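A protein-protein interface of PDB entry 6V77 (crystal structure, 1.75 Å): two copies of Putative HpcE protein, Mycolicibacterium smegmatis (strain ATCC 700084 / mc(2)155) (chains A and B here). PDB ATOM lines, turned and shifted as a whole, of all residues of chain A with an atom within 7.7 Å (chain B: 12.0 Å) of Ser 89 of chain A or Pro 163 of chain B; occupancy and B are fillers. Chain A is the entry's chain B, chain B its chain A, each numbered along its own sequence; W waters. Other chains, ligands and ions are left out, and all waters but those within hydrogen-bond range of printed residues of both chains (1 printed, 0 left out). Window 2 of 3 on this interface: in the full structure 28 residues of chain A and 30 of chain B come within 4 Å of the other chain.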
ATOM      1  N   LEU A  77     -13.769  -1.476 -30.159  1.00  0.00           N
ATOM      2  CA  LEU A  77     -12.316  -1.356 -30.036  1.00  0.00           C
ATOM      3  C   LEU A  77     -11.547  -2.068 -31.140  1.00  0.00           C
ATOM      4  O   LEU A  77     -10.880  -3.073 -30.877  1.00  0.00           O
ATOM      5  CB  LEU A  77     -11.856  -1.896 -28.682  1.00  0.00           C
ATOM      6  CG  LEU A  77     -12.624  -1.339 -27.479  1.00  0.00           C
ATOM      7  CD1 LEU A  77     -12.082  -1.926 -26.191  1.00  0.00           C
ATOM      8  CD2 LEU A  77     -12.582   0.188 -27.443  1.00  0.00           C
ATOM      9  N   ASP A  80      -6.384   0.788 -32.657  1.00  0.00           N
ATOM     10  CA  ASP A  80      -5.643   0.840 -31.398  1.00  0.00           C
ATOM     11  C   ASP A  80      -5.851   2.166 -30.684  1.00  0.00           C
ATOM     12  O   ASP A  80      -6.014   2.197 -29.458  1.00  0.00           O
ATOM     13  CB  ASP A  80      -4.151   0.614 -31.624  1.00  0.00           C
ATOM     14  CG  ASP A  80      -3.399   0.417 -30.313  1.00  0.00           C
ATOM     15  OD1 ASP A  80      -3.922  -0.314 -29.437  1.00  0.00           O
ATOM     16  OD2 ASP A  80      -2.298   0.989 -30.153  1.00  0.00           O
ATOM     17  N   ALA A  83      -9.133   2.223 -28.929  1.00  0.00           N
ATOM     18  CA  ALA A  83      -9.011   1.430 -27.707  1.00  0.00           C
ATOM     19  C   ALA A  83      -8.368   2.240 -26.582  1.00  0.00           C
ATOM     20  O   ALA A  83      -8.870   2.263 -25.448  1.00  0.00           O
ATOM     21  CB  ALA A  83      -8.202   0.163 -27.986  1.00  0.00           C
ATOM     22  N   THR A  84      -7.264   2.932 -26.884  1.00  0.00           N
ATOM     23  CA  THR A  84      -6.579   3.717 -25.859  1.00  0.00           C
ATOM     24  C   THR A  84      -7.495   4.781 -25.266  1.00  0.00           C
ATOM     25  O   THR A  84      -7.500   5.001 -24.051  1.00  0.00           O
ATOM     26  CB  THR A  84      -5.331   4.394 -26.440  1.00  0.00           C
ATOM     27  OG1 THR A  84      -4.523   3.430 -27.129  1.00  0.00           O
ATOM     28  CG2 THR A  84      -4.521   5.032 -25.337  1.00  0.00           C
ATOM     29  N   SER A  86     -10.730   4.874 -25.068  1.00  0.00           N
ATOM     30  CA  SER A  86     -11.916   4.356 -24.406  1.00  0.00           C
ATOM     31  C   SER A  86     -11.708   4.115 -22.920  1.00  0.00           C
ATOM     32  O   SER A  86     -12.693   3.907 -22.203  1.00  0.00           O
ATOM     33  CB  SER A  86     -12.334   3.038 -25.046  1.00  0.00           C
ATOM     34  OG  SER A  86     -11.422   2.045 -24.626  1.00  0.00           O
ATOM     35  N   GLY A  87     -10.463   4.108 -22.450  1.00  0.00           N
ATOM     36  CA  GLY A  87     -10.167   3.741 -21.082  1.00  0.00           C
ATOM     37  C   GLY A  87     -10.082   2.252 -20.844  1.00  0.00           C
ATOM     38  O   GLY A  87      -9.738   1.834 -19.728  1.00  0.00           O
ATOM     39  N   LEU A  88     -10.373   1.438 -21.853  1.00  0.00           N
ATOM     40  CA  LEU A  88     -10.346  -0.011 -21.736  1.00  0.00           C
ATOM     41  C   LEU A  88      -9.045  -0.566 -22.304  1.00  0.00           C
ATOM     42  O   LEU A  88      -8.322   0.107 -23.044  1.00  0.00           O
ATOM     43  CB  LEU A  88     -11.534  -0.627 -22.471  1.00  0.00           C
ATOM     44  CG  LEU A  88     -12.913  -0.175 -21.982  1.00  0.00           C
ATOM     45  CD1 LEU A  88     -13.986  -0.558 -22.990  1.00  0.00           C
ATOM     46  CD2 LEU A  88     -13.222  -0.779 -20.621  1.00  0.00           C
ATOM     47  N   SER A  89      -8.766  -1.818 -21.949  1.00  0.00           N
ATOM     48  CA  SER A  89      -7.608  -2.528 -22.471  1.00  0.00           C
ATOM     49  C   SER A  89      -7.792  -2.862 -23.951  1.00  0.00           C
ATOM     50  O   SER A  89      -8.914  -2.987 -24.448  1.00  0.00           O
ATOM     51  CB  SER A  89      -7.378  -3.813 -21.671  1.00  0.00           C
ATOM     52  OG  SER A  89      -6.932  -3.490 -20.365  1.00  0.00           O
ATOM     53  N   LYS A  90      -6.667  -2.995 -24.657  1.00  0.00           N
ATOM     54  CA  LYS A  90      -6.717  -3.360 -26.061  1.00  0.00           C
ATOM     55  C   LYS A  90      -7.191  -4.804 -26.181  1.00  0.00           C
ATOM     56  O   LYS A  90      -6.745  -5.659 -25.410  1.00  0.00           O
ATOM     57  CB  LYS A  90      -5.342  -3.211 -26.716  1.00  0.00           C
ATOM     58  N   PRO A  91      -8.090  -5.097 -27.119  1.00  0.00           N
ATOM     59  CA  PRO A  91      -8.639  -6.452 -27.227  1.00  0.00           C
ATOM     60  C   PRO A  91      -7.700  -7.408 -27.941  1.00  0.00           C
ATOM     61  O   PRO A  91      -6.933  -7.028 -28.829  1.00  0.00           O
ATOM     62  CB  PRO A  91      -9.918  -6.239 -28.044  1.00  0.00           C
ATOM     63  CG  PRO A  91      -9.557  -5.112 -28.956  1.00  0.00           C
ATOM     64  CD  PRO A  91      -8.698  -4.180 -28.105  1.00  0.00           C
ATOM     65  N   GLU A  92      -7.780  -8.675 -27.537  1.00  0.00           N
ATOM     66  CA  GLU A  92      -7.077  -9.759 -28.207  1.00  0.00           C
ATOM     67  C   GLU A  92      -7.940 -10.480 -29.234  1.00  0.00           C
ATOM     68  O   GLU A  92      -7.403 -11.201 -30.078  1.00  0.00           O
ATOM     69  CB  GLU A  92      -6.566 -10.773 -27.178  1.00  0.00           C
ATOM     70  N   HIS A  93      -9.253 -10.312 -29.172  1.00  0.00           N
ATOM     71  CA  HIS A  93     -10.181 -10.842 -30.156  1.00  0.00           C
ATOM     72  C   HIS A  93     -11.240  -9.782 -30.401  1.00  0.00           C
ATOM     73  O   HIS A  93     -11.447  -8.906 -29.557  1.00  0.00           O
ATOM     74  CB  HIS A  93     -10.837 -12.140 -29.667  1.00  0.00           C
ATOM     75  CG  HIS A  93      -9.848 -13.210 -29.339  1.00  0.00           C
ATOM     76  ND1 HIS A  93      -9.303 -14.037 -30.299  1.00  0.00           N
ATOM     77  CD2 HIS A  93      -9.277 -13.565 -28.164  1.00  0.00           C
ATOM     78  CE1 HIS A  93      -8.450 -14.867 -29.726  1.00  0.00           C
ATOM     79  NE2 HIS A  93      -8.415 -14.601 -28.432  1.00  0.00           N
ATOM     80  N   VAL A  95     -14.395  -7.599 -30.304  1.00  0.00           N
ATOM     81  CA  VAL A  95     -15.482  -7.339 -29.365  1.00  0.00           C
ATOM     82  C   VAL A  95     -16.756  -7.182 -30.189  1.00  0.00           C
ATOM     83  O   VAL A  95     -16.835  -6.292 -31.039  1.00  0.00           O
ATOM     84  CB  VAL A  95     -15.199  -6.070 -28.545  1.00  0.00           C
ATOM     85  CG1 VAL A  95     -16.355  -5.772 -27.613  1.00  0.00           C
ATOM     86  CG2 VAL A  95     -13.890  -6.204 -27.766  1.00  0.00           C
ATOM     87  N   PRO A 165     -21.931  -3.981 -18.375  1.00  0.00           N
ATOM     88  CA  PRO A 165     -22.535  -3.132 -19.422  1.00  0.00           C
ATOM     89  C   PRO A 165     -22.494  -3.766 -20.803  1.00  0.00           C
ATOM     90  O   PRO A 165     -21.427  -4.116 -21.325  1.00  0.00           O
ATOM     91  CB  PRO A 165     -21.689  -1.851 -19.376  1.00  0.00           C
ATOM     92  CG  PRO A 165     -20.435  -2.231 -18.666  1.00  0.00           C
ATOM     93  CD  PRO A 165     -20.825  -3.288 -17.684  1.00  0.00           C
ATOM     94  N   PHE A 167     -23.472  -3.144 -24.853  1.00  0.00           N
ATOM     95  CA  PHE A 167     -23.420  -1.927 -25.655  1.00  0.00           C
ATOM     96  C   PHE A 167     -24.558  -1.763 -26.663  1.00  0.00           C
ATOM     97  O   PHE A 167     -24.747  -0.650 -27.166  1.00  0.00           O
ATOM     98  CB  PHE A 167     -22.086  -1.856 -26.414  1.00  0.00           C
ATOM     99  CG  PHE A 167     -20.861  -1.794 -25.521  1.00  0.00           C
ATOM    100  CD1 PHE A 167     -20.977  -1.545 -24.162  1.00  0.00           C
ATOM    101  CD2 PHE A 167     -19.587  -1.956 -26.061  1.00  0.00           C
ATOM    102  CE1 PHE A 167     -19.851  -1.471 -23.344  1.00  0.00           C
ATOM    103  CE2 PHE A 167     -18.450  -1.868 -25.239  1.00  0.00           C
ATOM    104  CZ  PHE A 167     -18.588  -1.631 -23.890  1.00  0.00           C
ATOM    105  N   ILE A 215      -7.414  -3.235 -36.170  1.00  0.00           N
ATOM    106  CA  ILE A 215      -6.716  -4.287 -35.439  1.00  0.00           C
ATOM    107  C   ILE A 215      -7.058  -5.642 -36.038  1.00  0.00           C
ATOM    108  O   ILE A 215      -6.186  -6.485 -36.272  1.00  0.00           O
ATOM    109  CB  ILE A 215      -7.078  -4.230 -33.944  1.00  0.00           C
ATOM    110  CG1 ILE A 215      -6.621  -2.907 -33.330  1.00  0.00           C
ATOM    111  CG2 ILE A 215      -6.457  -5.406 -33.199  1.00  0.00           C
ATOM    112  CD1 ILE A 215      -7.171  -2.667 -31.913  1.00  0.00           C
ATOM    113  N   ARG B 156     -19.168 -19.986 -21.545  1.00  0.00           N
ATOM    114  CA  ARG B 156     -18.834 -18.945 -20.572  1.00  0.00           C
ATOM    115  C   ARG B 156     -17.453 -18.340 -20.799  1.00  0.00           C
ATOM    116  O   ARG B 156     -17.229 -17.180 -20.441  1.00  0.00           O
ATOM    117  CB  ARG B 156     -18.916 -19.485 -19.141  1.00  0.00           C
ATOM    118  CG  ARG B 156     -20.295 -19.993 -18.720  1.00  0.00           C
ATOM    119  CD  ARG B 156     -21.355 -18.873 -18.683  1.00  0.00           C
ATOM    120  NE  ARG B 156     -22.556 -19.288 -17.951  1.00  0.00           N
ATOM    121  CZ  ARG B 156     -23.736 -18.677 -18.029  1.00  0.00           C
ATOM    122  NH1 ARG B 156     -23.885 -17.616 -18.807  1.00  0.00           N
ATOM    123  NH2 ARG B 156     -24.771 -19.124 -17.318  1.00  0.00           N
ATOM    124  N   ASP B 157     -16.504 -19.104 -21.342  1.00  0.00           N
ATOM    125  CA  ASP B 157     -15.179 -18.544 -21.567  1.00  0.00           C
ATOM    126  C   ASP B 157     -15.250 -17.365 -22.532  1.00  0.00           C
ATOM    127  O   ASP B 157     -14.787 -16.261 -22.220  1.00  0.00           O
ATOM    128  CB  ASP B 157     -14.228 -19.617 -22.106  1.00  0.00           C
ATOM    129  CG  ASP B 157     -14.058 -20.788 -21.154  1.00  0.00           C
ATOM    130  OD1 ASP B 157     -14.416 -20.665 -19.961  1.00  0.00           O
ATOM    131  OD2 ASP B 157     -13.554 -21.835 -21.610  1.00  0.00           O
ATOM    132  N   LEU B 158     -15.842 -17.580 -23.710  1.00  0.00           N
ATOM    133  CA  LEU B 158     -15.986 -16.479 -24.660  1.00  0.00           C
ATOM    134  C   LEU B 158     -16.902 -15.393 -24.114  1.00  0.00           C
ATOM    135  O   LEU B 158     -16.672 -14.205 -24.362  1.00  0.00           O
ATOM    136  CB  LEU B 158     -16.507 -17.000 -26.009  1.00  0.00           C
ATOM    137  CG  LEU B 158     -16.794 -16.010 -27.145  1.00  0.00           C
ATOM    138  CD1 LEU B 158     -15.530 -15.246 -27.494  1.00  0.00           C
ATOM    139  CD2 LEU B 158     -17.358 -16.731 -28.384  1.00  0.00           C
ATOM    140  N   GLN B 159     -17.912 -15.770 -23.330  1.00  0.00           N
ATOM    141  CA  GLN B 159     -18.892 -14.783 -22.881  1.00  0.00           C
ATOM    142  C   GLN B 159     -18.277 -13.715 -21.984  1.00  0.00           C
ATOM    143  O   GLN B 159     -18.633 -12.537 -22.092  1.00  0.00           O
ATOM    144  CB  GLN B 159     -20.038 -15.466 -22.140  1.00  0.00           C
ATOM    145  CG  GLN B 159     -21.158 -14.491 -21.788  1.00  0.00           C
ATOM    146  CD  GLN B 159     -22.143 -15.042 -20.765  1.00  0.00           C
ATOM    147  OE1 GLN B 159     -22.352 -16.249 -20.678  1.00  0.00           O
ATOM    148  NE2 GLN B 159     -22.751 -14.146 -19.981  1.00  0.00           N
ATOM    149  N   LEU B 160     -17.368 -14.101 -21.085  1.00  0.00           N
ATOM    150  CA  LEU B 160     -16.926 -13.211 -20.017  1.00  0.00           C
ATOM    151  C   LEU B 160     -15.516 -12.669 -20.209  1.00  0.00           C
ATOM    152  O   LEU B 160     -15.056 -11.869 -19.388  1.00  0.00           O
ATOM    153  CB  LEU B 160     -17.028 -13.936 -18.667  1.00  0.00           C
ATOM    154  CG  LEU B 160     -18.422 -14.467 -18.307  1.00  0.00           C
ATOM    155  CD1 LEU B 160     -18.389 -15.316 -17.033  1.00  0.00           C
ATOM    156  CD2 LEU B 160     -19.430 -13.329 -18.161  1.00  0.00           C
ATOM    157  N   ALA B 161     -14.831 -13.049 -21.277  1.00  0.00           N
ATOM    158  CA  ALA B 161     -13.435 -12.692 -21.436  1.00  0.00           C
ATOM    159  C   ALA B 161     -13.275 -11.295 -22.034  1.00  0.00           C
ATOM    160  O   ALA B 161     -14.162 -10.764 -22.709  1.00  0.00           O
ATOM    161  CB  ALA B 161     -12.730 -13.719 -22.325  1.00  0.00           C
ATOM    162  N   GLY B 162     -12.110 -10.704 -21.781  1.00  0.00           N
ATOM    163  CA  GLY B 162     -11.691  -9.514 -22.483  1.00  0.00           C
ATOM    164  C   GLY B 162     -12.172  -8.242 -21.822  1.00  0.00           C
ATOM    165  O   GLY B 162     -12.798  -8.264 -20.759  1.00  0.00           O
ATOM    166  N   PRO B 163     -11.879  -7.100 -22.440  1.00  0.00           N
ATOM    167  CA  PRO B 163     -12.366  -5.829 -21.894  1.00  0.00           C
ATOM    168  C   PRO B 163     -13.858  -5.688 -22.157  1.00  0.00           C
ATOM    169  O   PRO B 163     -14.332  -5.967 -23.261  1.00  0.00           O
ATOM    170  CB  PRO B 163     -11.550  -4.779 -22.656  1.00  0.00           C
ATOM    171  CG  PRO B 163     -11.248  -5.435 -23.976  1.00  0.00           C
ATOM    172  CD  PRO B 163     -11.135  -6.919 -23.704  1.00  0.00           C
ATOM    173  N   ALA B 164     -14.597  -5.274 -21.121  1.00  0.00           N
ATOM    174  CA  ALA B 164     -16.037  -5.051 -21.192  1.00  0.00           C
ATOM    175  C   ALA B 164     -16.712  -6.188 -21.949  1.00  0.00           C
ATOM    176  O   ALA B 164     -17.167  -5.987 -23.085  1.00  0.00           O
ATOM    177  CB  ALA B 164     -16.344  -3.716 -21.871  1.00  0.00           C
ATOM    178  N   PRO B 165     -16.750  -7.391 -21.381  1.00  0.00           N
ATOM    179  CA  PRO B 165     -17.240  -8.551 -22.140  1.00  0.00           C
ATOM    180  C   PRO B 165     -18.652  -8.325 -22.655  1.00  0.00           C
ATOM    181  O   PRO B 165     -19.540  -7.901 -21.915  1.00  0.00           O
ATOM    182  CB  PRO B 165     -17.186  -9.693 -21.120  1.00  0.00           C
ATOM    183  CG  PRO B 165     -17.144  -9.014 -19.785  1.00  0.00           C
ATOM    184  CD  PRO B 165     -16.375  -7.755 -20.006  1.00  0.00           C
ATOM    185  N   GLN B 166     -18.842  -8.608 -23.944  1.00  0.00           N
ATOM    186  CA  GLN B 166     -20.126  -8.509 -24.619  1.00  0.00           C
ATOM    187  C   GLN B 166     -20.631  -9.924 -24.866  1.00  0.00           C
ATOM    188  O   GLN B 166     -19.916 -10.738 -25.457  1.00  0.00           O
ATOM    189  CB  GLN B 166     -19.970  -7.742 -25.939  1.00  0.00           C
ATOM    190  CG  GLN B 166     -19.417  -6.324 -25.728  1.00  0.00           C
ATOM    191  CD  GLN B 166     -20.339  -5.467 -24.896  1.00  0.00           C
ATOM    192  OE1 GLN B 166     -21.489  -5.230 -25.270  1.00  0.00           O
ATOM    193  NE2 GLN B 166     -19.842  -4.995 -23.758  1.00  0.00           N
ATOM    194  N   PHE B 167     -21.860 -10.209 -24.431  1.00  0.00           N
ATOM    195  CA  PHE B 167     -22.291 -11.595 -24.229  1.00  0.00           C
ATOM    196  C   PHE B 167     -22.833 -12.305 -25.474  1.00  0.00           C
ATOM    197  O   PHE B 167     -23.013 -13.522 -25.415  1.00  0.00           O
ATOM    198  CB  PHE B 167     -23.384 -11.661 -23.149  1.00  0.00           C
ATOM    199  CG  PHE B 167     -22.941 -11.190 -21.778  1.00  0.00           C
ATOM    200  CD1 PHE B 167     -21.603 -11.076 -21.457  1.00  0.00           C
ATOM    201  CD2 PHE B 167     -23.888 -10.909 -20.801  1.00  0.00           C
ATOM    202  CE1 PHE B 167     -21.198 -10.657 -20.195  1.00  0.00           C
ATOM    203  CE2 PHE B 167     -23.491 -10.492 -19.531  1.00  0.00           C
ATOM    204  CZ  PHE B 167     -22.142 -10.362 -19.231  1.00  0.00           C
ATOM    205  N   SER B 168     -23.107 -11.616 -26.592  1.00  0.00           N
ATOM    206  CA  SER B 168     -23.973 -12.231 -27.612  1.00  0.00           C
ATOM    207  C   SER B 168     -23.306 -13.406 -28.321  1.00  0.00           C
ATOM    208  O   SER B 168     -23.942 -14.446 -28.542  1.00  0.00           O
ATOM    209  CB  SER B 168     -24.404 -11.193 -28.649  1.00  0.00           C
ATOM    210  OG  SER B 168     -25.129 -10.140 -28.019  1.00  0.00           O
ATOM    211  N   LEU B 169     -22.049 -13.249 -28.742  1.00  0.00           N
ATOM    212  CA  LEU B 169     -21.453 -14.279 -29.598  1.00  0.00           C
ATOM    213  C   LEU B 169     -21.366 -15.622 -28.877  1.00  0.00           C
ATOM    214  O   LEU B 169     -21.641 -16.682 -29.469  1.00  0.00           O
ATOM    215  CB  LEU B 169     -20.067 -13.833 -30.064  1.00  0.00           C
ATOM    216  CG  LEU B 169     -19.521 -14.528 -31.321  1.00  0.00           C
ATOM    217  CD1 LEU B 169     -20.422 -14.277 -32.536  1.00  0.00           C
ATOM    218  CD2 LEU B 169     -18.110 -14.026 -31.610  1.00  0.00           C
HETATM  219  O   HOH W   1     -19.576  -5.942 -19.970  1.00  0.00           O
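Of the 14 printed residues of chain B, 3 touch a printed residue of chain A.
Printed residues of chain B that touch a printed residue of chain A: Pro 163, Ala 164 and Gln 166.
Hydrophobic or aromatic side chains of chain B within 4 Å of the printed part of chain A: Pro 163 and Ala 164.
Along chain A the printed residues that touch a printed residue of chain B span positions 89 to 167.
Among the printed residues, 5 pairs touch across the chains.
Among the printed residues, no Asp or Glu carboxylate lies within 4 Å of a Lys or Arg side-chain nitrogen of the other chain.
Water W1 lies within hydrogen-bond range of O of Pro 165 of chain B and O of Pro 165 of chain A.
The backbone carbonyl oxygen (O) of Ala 164 of chain B is in hydrogen-bond range of the side-chain amide nitrogen (NE2) of Gln 166 of chain B (2.9 Å).
Positions printed for both chains: 165 and 167.
Of the 5 pairs that touch across the chains among the printed residues, none has its exchanged pair printed and touching as well.
The side-chain amide nitrogen of Gln 166 of chain B sits at hydrogen-bond distance from the backbone carbonyl oxygen of Pro 165 of chain A.
The side-chain amide oxygen of Gln 166 of chain B is in hydrogen-bond range of the backbone NH of Phe 167 of chain A (2.9 Å).
Ser 89 of chain A touches Pro 163 of chain B.
Val 95 of chain A touches Gln 166 of chain B (CG1 to CG, 3.6 Å).
CB of Ala 164 of chain B touches CZ of Phe 167 of chain A (3.7 Å).
No residue of chain B comes within 4 Å of Gly 87 of chain A.
Of chain B, only Pro 163 comes within 4 Å of Ser 89 of chain A.
No residue of chain B comes within 4 Å of Lys 90 of chain A.
Of the printed residues of chain B, Val 95 of chain A touches Gln 166 (3.6 Å).
Of the printed residues of chain B, Pro 165 of chain A touches Gln 166.
Printed residues of chain B within 4 Å of Phe 167 of chain A: Ala 164 (3.7 Å) and Gln 166 (2.9 Å).
Pro 163 of chain B touches just one residue of chain A: Ser 89 (3.4 Å).
Of chain A, only Phe 167 (3.7 Å) comes within 4 Å of Ala 164 of chain B.
The nearest residue of chain B that does not touch Ser 89 of chain A is Gly 162 of chain B (6.5 Å).
The nearest residue of chain A that does not touch Pro 163 of chain B is Leu 88 of chain A (4.2 Å).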
